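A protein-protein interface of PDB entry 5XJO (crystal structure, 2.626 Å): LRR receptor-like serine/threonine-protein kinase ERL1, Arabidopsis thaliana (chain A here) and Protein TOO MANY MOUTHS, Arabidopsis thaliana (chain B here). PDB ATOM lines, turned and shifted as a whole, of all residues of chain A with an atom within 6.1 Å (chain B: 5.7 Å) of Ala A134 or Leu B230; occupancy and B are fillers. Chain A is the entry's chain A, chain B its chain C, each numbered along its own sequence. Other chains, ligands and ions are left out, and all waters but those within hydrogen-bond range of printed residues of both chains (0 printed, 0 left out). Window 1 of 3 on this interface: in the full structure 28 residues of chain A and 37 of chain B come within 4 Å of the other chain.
OE1 of Gln B253 sits at hydrogen-bond distance from OG of Ser A157. NE2 of Gln A138 lies close to OD2 of Asp B232. O of Thr A137 sits at hydrogen-bond distance from NZ of Lys B206 (2.7 Å).
The backbone NH of Gln B253 is in hydrogen-bond range of the backbone carbonyl oxygen of Val B229, at 2.7 Å. The backbone carbonyl oxygen (O) of Gln B253 lies within hydrogen-bond range of the backbone NH (N) of Ile B280, at 2.9 Å. The backbone NH (N) of Ala B254 is in hydrogen-bond range of the backbone carbonyl oxygen (O) of Val B229, at 3.2 Å. The backbone carbonyl oxygen (O) of Leu B230 sits at hydrogen-bond distance from the backbone NH (N) of Ile B207 (3.0 Å). O of Ala A134 sits at hydrogen-bond distance from OG1 of Thr A137, at 2.8 Å. N of Met B256 sits at hydrogen-bond distance from O of Leu B231, at 3.0 Å.
Ala A134 touches Leu B230 (O to CD1, 3.8 Å). Thr A135 touches Ile B280. OD2 of Asp B208 touches NE2 of Gln A138, 3.8 Å away. Gln A138 touches Leu B230 (OE1 to CD1, 3.8 Å). OE1 of Gln A138 touches CE of Met B256 (3.3 Å). CG1 of Val B229 touches OG of Ser A157, 3.4 Å away. CD2 of Leu A159 touches O of Ile B205, at 3.9 Å. Leu A159 touches Lys B206. CB of Leu B230 touches CD2 of Leu A159, at 3.8 Å.
Ala A134 touches just one residue of chain B: Leu B230 (3.8 Å). Printed residues of chain B within 4 Å of Leu A159: Ile B205, Lys B206 and Leu B230. Of the printed residues of chain A, Lys B206 touches Thr A137 and Leu A159. Printed residues of chain A within 4 Å of Gln B253: Ser A157. The nearest residue of chain B that does not touch Ala A134 is Gln B253 (4.3 Å). The nearest printed residue of chain A that does not touch Gln B253 is Ala A134 (4.3 Å).
Of the 15 printed residues of chain B, 9 touch a printed residue of chain A. Of the 9 printed residues of chain A, 6 touch a printed residue of chain B. Hydrophobic or aromatic side chains of chain A within 4 Å of the printed part of chain B: Ala A134 and Leu A159. Along chain A the printed residues that touch a printed residue of chain B span positions 134 to 159.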
ATOM      1  N   VAL A 132      12.986 -25.239 -20.313  1.00  0.00           N
ATOM      2  CA  VAL A 132      13.285 -23.907 -19.802  1.00  0.00           C
ATOM      3  C   VAL A 132      12.984 -24.056 -18.321  1.00  0.00           C
ATOM      4  O   VAL A 132      11.821 -24.262 -17.959  1.00  0.00           O
ATOM      5  CB  VAL A 132      12.468 -22.801 -20.489  1.00  0.00           C
ATOM      6  CG1 VAL A 132      12.660 -21.473 -19.752  1.00  0.00           C
ATOM      7  CG2 VAL A 132      12.894 -22.667 -21.964  1.00  0.00           C
ATOM      8  N   PRO A 133      13.993 -24.094 -17.459  1.00  0.00           N
ATOM      9  CA  PRO A 133      13.779 -24.530 -16.073  1.00  0.00           C
ATOM     10  C   PRO A 133      13.133 -23.458 -15.198  1.00  0.00           C
ATOM     11  O   PRO A 133      13.218 -22.252 -15.447  1.00  0.00           O
ATOM     12  CB  PRO A 133      15.200 -24.855 -15.585  1.00  0.00           C
ATOM     13  CG  PRO A 133      16.089 -23.934 -16.396  1.00  0.00           C
ATOM     14  CD  PRO A 133      15.419 -23.806 -17.738  1.00  0.00           C
ATOM     15  N   ALA A 134      12.463 -23.935 -14.147  1.00  0.00           N
ATOM     16  CA  ALA A 134      11.850 -23.015 -13.198  1.00  0.00           C
ATOM     17  C   ALA A 134      12.884 -22.281 -12.345  1.00  0.00           C
ATOM     18  O   ALA A 134      12.565 -21.219 -11.821  1.00  0.00           O
ATOM     19  CB  ALA A 134      10.863 -23.768 -12.319  1.00  0.00           C
ATOM     20  N   THR A 135      14.107 -22.817 -12.203  1.00  0.00           N
ATOM     21  CA  THR A 135      15.153 -22.167 -11.419  1.00  0.00           C
ATOM     22  C   THR A 135      15.509 -20.774 -11.929  1.00  0.00           C
ATOM     23  O   THR A 135      16.054 -19.966 -11.170  1.00  0.00           O
ATOM     24  CB  THR A 135      16.417 -23.053 -11.389  1.00  0.00           C
ATOM     25  OG1 THR A 135      17.047 -23.126 -12.685  1.00  0.00           O
ATOM     26  CG2 THR A 135      16.070 -24.422 -10.940  1.00  0.00           C
ATOM     27  N   LEU A 136      15.239 -20.476 -13.204  1.00  0.00           N
ATOM     28  CA  LEU A 136      15.457 -19.111 -13.669  1.00  0.00           C
ATOM     29  C   LEU A 136      14.411 -18.142 -13.192  1.00  0.00           C
ATOM     30  O   LEU A 136      14.508 -16.956 -13.530  1.00  0.00           O
ATOM     31  CB  LEU A 136      15.491 -19.005 -15.201  1.00  0.00           C
ATOM     32  CG  LEU A 136      16.207 -19.924 -16.189  1.00  0.00           C
ATOM     33  CD1 LEU A 136      15.604 -19.723 -17.640  1.00  0.00           C
ATOM     34  CD2 LEU A 136      17.724 -19.654 -16.097  1.00  0.00           C
ATOM     35  N   THR A 137      13.452 -18.574 -12.395  1.00  0.00           N
ATOM     36  CA  THR A 137      12.583 -17.647 -11.717  1.00  0.00           C
ATOM     37  C   THR A 137      13.100 -17.313 -10.309  1.00  0.00           C
ATOM     38  O   THR A 137      12.381 -16.688  -9.525  1.00  0.00           O
ATOM     39  CB  THR A 137      11.173 -18.215 -11.673  1.00  0.00           C
ATOM     40  OG1 THR A 137      11.050 -19.169 -10.596  1.00  0.00           O
ATOM     41  CG2 THR A 137      10.854 -18.904 -12.982  1.00  0.00           C
ATOM     42  N   GLN A 138      14.328 -17.727  -9.989  1.00  0.00           N
ATOM     43  CA  GLN A 138      15.045 -17.371  -8.770  1.00  0.00           C
ATOM     44  C   GLN A 138      16.299 -16.561  -9.088  1.00  0.00           C
ATOM     45  O   GLN A 138      17.288 -16.608  -8.346  1.00  0.00           O
ATOM     46  CB  GLN A 138      15.420 -18.604  -7.947  1.00  0.00           C
ATOM     47  CG  GLN A 138      14.237 -19.378  -7.397  1.00  0.00           C
ATOM     48  CD  GLN A 138      14.628 -20.776  -6.887  1.00  0.00           C
ATOM     49  OE1 GLN A 138      15.160 -21.602  -7.647  1.00  0.00           O
ATOM     50  NE2 GLN A 138      14.345 -21.050  -5.609  1.00  0.00           N
ATOM     51  N   SER A 157       6.236 -22.892 -18.380  1.00  0.00           N
ATOM     52  CA  SER A 157       5.540 -22.900 -17.113  1.00  0.00           C
ATOM     53  C   SER A 157       5.022 -21.492 -16.820  1.00  0.00           C
ATOM     54  O   SER A 157       5.716 -20.484 -17.039  1.00  0.00           O
ATOM     55  CB  SER A 157       6.459 -23.418 -16.006  1.00  0.00           C
ATOM     56  OG  SER A 157       5.701 -24.113 -15.016  1.00  0.00           O
ATOM     57  N   LEU A 159       4.761 -20.153 -14.186  1.00  0.00           N
ATOM     58  CA  LEU A 159       5.606 -19.513 -13.191  1.00  0.00           C
ATOM     59  C   LEU A 159       6.541 -18.516 -13.837  1.00  0.00           C
ATOM     60  O   LEU A 159       6.808 -17.453 -13.271  1.00  0.00           O
ATOM     61  CB  LEU A 159       6.413 -20.558 -12.419  1.00  0.00           C
ATOM     62  CG  LEU A 159       7.045 -19.995 -11.154  1.00  0.00           C
ATOM     63  CD1 LEU A 159       6.091 -18.994 -10.427  1.00  0.00           C
ATOM     64  CD2 LEU A 159       7.408 -21.146 -10.235  1.00  0.00           C
ATOM     65  N   ILE B 205       1.572 -21.393  -6.542  1.00  0.00           N
ATOM     66  CA  ILE B 205       2.394 -22.008  -7.579  1.00  0.00           C
ATOM     67  C   ILE B 205       3.878 -21.925  -7.265  1.00  0.00           C
ATOM     68  O   ILE B 205       4.669 -22.629  -7.906  1.00  0.00           O
ATOM     69  CB  ILE B 205       2.111 -21.386  -8.962  1.00  0.00           C
ATOM     70  CG1 ILE B 205       2.467 -19.906  -8.951  1.00  0.00           C
ATOM     71  CG2 ILE B 205       0.637 -21.500  -9.339  1.00  0.00           C
ATOM     72  CD1 ILE B 205       1.999 -19.170 -10.194  1.00  0.00           C
ATOM     73  N   LYS B 206       4.285 -21.112  -6.294  1.00  0.00           N
ATOM     74  CA  LYS B 206       5.692 -20.945  -5.953  1.00  0.00           C
ATOM     75  C   LYS B 206       5.822 -20.575  -4.488  1.00  0.00           C
ATOM     76  O   LYS B 206       5.192 -19.613  -4.050  1.00  0.00           O
ATOM     77  CB  LYS B 206       6.348 -19.857  -6.794  1.00  0.00           C
ATOM     78  CG  LYS B 206       7.775 -19.532  -6.334  1.00  0.00           C
ATOM     79  CD  LYS B 206       8.358 -18.433  -7.164  1.00  0.00           C
ATOM     80  CE  LYS B 206       9.842 -18.370  -6.999  1.00  0.00           C
ATOM     81  NZ  LYS B 206      10.368 -17.317  -7.905  1.00  0.00           N
ATOM     82  N   ILE B 207       6.623 -21.336  -3.746  1.00  0.00           N
ATOM     83  CA  ILE B 207       6.968 -21.010  -2.373  1.00  0.00           C
ATOM     84  C   ILE B 207       8.480 -20.952  -2.273  1.00  0.00           C
ATOM     85  O   ILE B 207       9.149 -21.987  -2.335  1.00  0.00           O
ATOM     86  CB  ILE B 207       6.388 -22.011  -1.367  1.00  0.00           C
ATOM     87  CG1 ILE B 207       4.863 -22.038  -1.503  1.00  0.00           C
ATOM     88  CG2 ILE B 207       6.863 -21.667   0.078  1.00  0.00           C
ATOM     89  CD1 ILE B 207       4.190 -23.206  -0.815  1.00  0.00           C
ATOM     90  N   ASP B 208       9.019 -19.747  -2.117  1.00  0.00           N
ATOM     91  CA  ASP B 208      10.453 -19.543  -1.916  1.00  0.00           C
ATOM     92  C   ASP B 208      10.654 -19.040  -0.488  1.00  0.00           C
ATOM     93  O   ASP B 208      10.466 -17.853  -0.202  1.00  0.00           O
ATOM     94  CB  ASP B 208      11.004 -18.552  -2.941  1.00  0.00           C
ATOM     95  CG  ASP B 208      12.513 -18.566  -3.016  1.00  0.00           C
ATOM     96  OD1 ASP B 208      13.152 -19.194  -2.150  1.00  0.00           O
ATOM     97  OD2 ASP B 208      13.070 -17.923  -3.930  1.00  0.00           O
ATOM     98  N   LEU B 228       1.313 -25.995  -7.294  1.00  0.00           N
ATOM     99  CA  LEU B 228       2.659 -25.604  -6.953  1.00  0.00           C
ATOM    100  C   LEU B 228       3.676 -26.153  -7.908  1.00  0.00           C
ATOM    101  O   LEU B 228       3.785 -27.316  -8.074  1.00  0.00           O
ATOM    102  CB  LEU B 228       2.942 -26.008  -5.523  1.00  0.00           C
ATOM    103  CG  LEU B 228       4.130 -25.447  -4.782  1.00  0.00           C
ATOM    104  CD1 LEU B 228       3.786 -24.068  -4.347  1.00  0.00           C
ATOM    105  CD2 LEU B 228       4.321 -26.319  -3.570  1.00  0.00           C
ATOM    106  N   VAL B 229       4.448 -25.272  -8.501  1.00  0.00           N
ATOM    107  CA  VAL B 229       5.423 -25.601  -9.523  1.00  0.00           C
ATOM    108  C   VAL B 229       6.825 -25.664  -8.937  1.00  0.00           C
ATOM    109  O   VAL B 229       7.593 -26.573  -9.258  1.00  0.00           O
ATOM    110  CB  VAL B 229       5.311 -24.563 -10.665  1.00  0.00           C
ATOM    111  CG1 VAL B 229       6.388 -24.756 -11.707  1.00  0.00           C
ATOM    112  CG2 VAL B 229       3.910 -24.589 -11.236  1.00  0.00           C
ATOM    113  N   LEU B 230       7.156 -24.716  -8.062  1.00  0.00           N
ATOM    114  CA  LEU B 230       8.456 -24.662  -7.402  1.00  0.00           C
ATOM    115  C   LEU B 230       8.318 -24.490  -5.886  1.00  0.00           C
ATOM    116  O   LEU B 230       7.504 -23.678  -5.406  1.00  0.00           O
ATOM    117  CB  LEU B 230       9.299 -23.519  -7.997  1.00  0.00           C
ATOM    118  CG  LEU B 230      10.711 -23.305  -7.444  1.00  0.00           C
ATOM    119  CD1 LEU B 230      11.677 -22.898  -8.572  1.00  0.00           C
ATOM    120  CD2 LEU B 230      10.710 -22.267  -6.352  1.00  0.00           C
ATOM    121  N   LEU B 231       9.124 -25.256  -5.135  1.00  0.00           N
ATOM    122  CA  LEU B 231       9.201 -25.149  -3.678  1.00  0.00           C
ATOM    123  C   LEU B 231      10.668 -25.163  -3.238  1.00  0.00           C
ATOM    124  O   LEU B 231      11.406 -26.116  -3.517  1.00  0.00           O
ATOM    125  CB  LEU B 231       8.429 -26.284  -3.014  1.00  0.00           C
ATOM    126  CG  LEU B 231       8.030 -26.235  -1.536  1.00  0.00           C
ATOM    127  CD1 LEU B 231       7.323 -27.506  -1.266  1.00  0.00           C
ATOM    128  CD2 LEU B 231       9.171 -26.127  -0.631  1.00  0.00           C
ATOM    129  N   ASP B 232      11.092 -24.123  -2.538  1.00  0.00           N
ATOM    130  CA  ASP B 232      12.489 -23.959  -2.168  1.00  0.00           C
ATOM    131  C   ASP B 232      12.568 -23.694  -0.672  1.00  0.00           C
ATOM    132  O   ASP B 232      12.202 -22.614  -0.212  1.00  0.00           O
ATOM    133  CB  ASP B 232      13.134 -22.818  -2.950  1.00  0.00           C
ATOM    134  CG  ASP B 232      14.647 -22.914  -2.955  1.00  0.00           C
ATOM    135  OD1 ASP B 232      15.211 -23.612  -2.057  1.00  0.00           O
ATOM    136  OD2 ASP B 232      15.274 -22.315  -3.871  1.00  0.00           O
ATOM    137  N   SER B 251       2.023 -30.795  -9.993  1.00  0.00           N
ATOM    138  CA  SER B 251       2.640 -29.773 -10.823  1.00  0.00           C
ATOM    139  C   SER B 251       4.079 -29.521 -10.407  1.00  0.00           C
ATOM    140  O   SER B 251       4.770 -28.724 -11.042  1.00  0.00           O
ATOM    141  CB  SER B 251       1.873 -28.446 -10.735  1.00  0.00           C
ATOM    142  OG  SER B 251       0.547 -28.573 -11.160  1.00  0.00           O
ATOM    143  N   LEU B 252       4.544 -30.163  -9.353  1.00  0.00           N
ATOM    144  CA  LEU B 252       5.829 -29.789  -8.808  1.00  0.00           C
ATOM    145  C   LEU B 252       6.934 -30.120  -9.805  1.00  0.00           C
ATOM    146  O   LEU B 252       7.114 -31.280 -10.200  1.00  0.00           O
ATOM    147  CB  LEU B 252       6.032 -30.495  -7.473  1.00  0.00           C
ATOM    148  CG  LEU B 252       7.228 -30.080  -6.628  1.00  0.00           C
ATOM    149  CD1 LEU B 252       6.839 -28.862  -5.808  1.00  0.00           C
ATOM    150  CD2 LEU B 252       7.616 -31.220  -5.692  1.00  0.00           C
ATOM    151  N   GLN B 253       7.636 -29.092 -10.263  1.00  0.00           N
ATOM    152  CA  GLN B 253       8.783 -29.332 -11.121  1.00  0.00           C
ATOM    153  C   GLN B 253      10.080 -29.264 -10.362  1.00  0.00           C
ATOM    154  O   GLN B 253      11.063 -29.867 -10.805  1.00  0.00           O
ATOM    155  CB  GLN B 253       8.841 -28.340 -12.292  1.00  0.00           C
ATOM    156  CG  GLN B 253       7.654 -28.372 -13.210  1.00  0.00           C
ATOM    157  CD  GLN B 253       7.726 -27.320 -14.302  1.00  0.00           C
ATOM    158  OE1 GLN B 253       6.700 -26.920 -14.842  1.00  0.00           O
ATOM    159  NE2 GLN B 253       8.927 -26.847 -14.612  1.00  0.00           N
ATOM    160  N   ALA B 254      10.095 -28.543  -9.238  1.00  0.00           N
ATOM    161  CA  ALA B 254      11.315 -28.341  -8.470  1.00  0.00           C
ATOM    162  C   ALA B 254      11.057 -28.428  -6.969  1.00  0.00           C
ATOM    163  O   ALA B 254      10.161 -27.766  -6.434  1.00  0.00           O
ATOM    164  CB  ALA B 254      11.938 -26.982  -8.832  1.00  0.00           C
ATOM    165  N   MET B 256      13.704 -28.111  -3.611  1.00  0.00           N
ATOM    166  CA  MET B 256      15.081 -27.930  -3.148  1.00  0.00           C
ATOM    167  C   MET B 256      15.110 -27.746  -1.632  1.00  0.00           C
ATOM    168  O   MET B 256      14.663 -26.717  -1.121  1.00  0.00           O
ATOM    169  CB  MET B 256      15.737 -26.741  -3.849  1.00  0.00           C
ATOM    170  CG  MET B 256      15.925 -26.884  -5.370  1.00  0.00           C
ATOM    171  SD  MET B 256      14.503 -26.426  -6.405  1.00  0.00           S
ATOM    172  CE  MET B 256      14.565 -24.627  -6.474  1.00  0.00           C
ATOM    173  N   ILE B 280      13.482 -31.403 -10.916  1.00  0.00           N
ATOM    174  CA  ILE B 280      14.654 -30.949 -10.161  1.00  0.00           C
ATOM    175  C   ILE B 280      14.486 -31.362  -8.702  1.00  0.00           C
ATOM    176  O   ILE B 280      13.520 -30.961  -8.045  1.00  0.00           O
ATOM    177  CB  ILE B 280      14.862 -29.430 -10.255  1.00  0.00           C
ATOM    178  CG1 ILE B 280      15.150 -28.988 -11.694  1.00  0.00           C
ATOM    179  CG2 ILE B 280      15.986 -29.017  -9.353  1.00  0.00           C
ATOM    180  CD1 ILE B 280      15.071 -27.523 -11.880  1.00  0.00           C
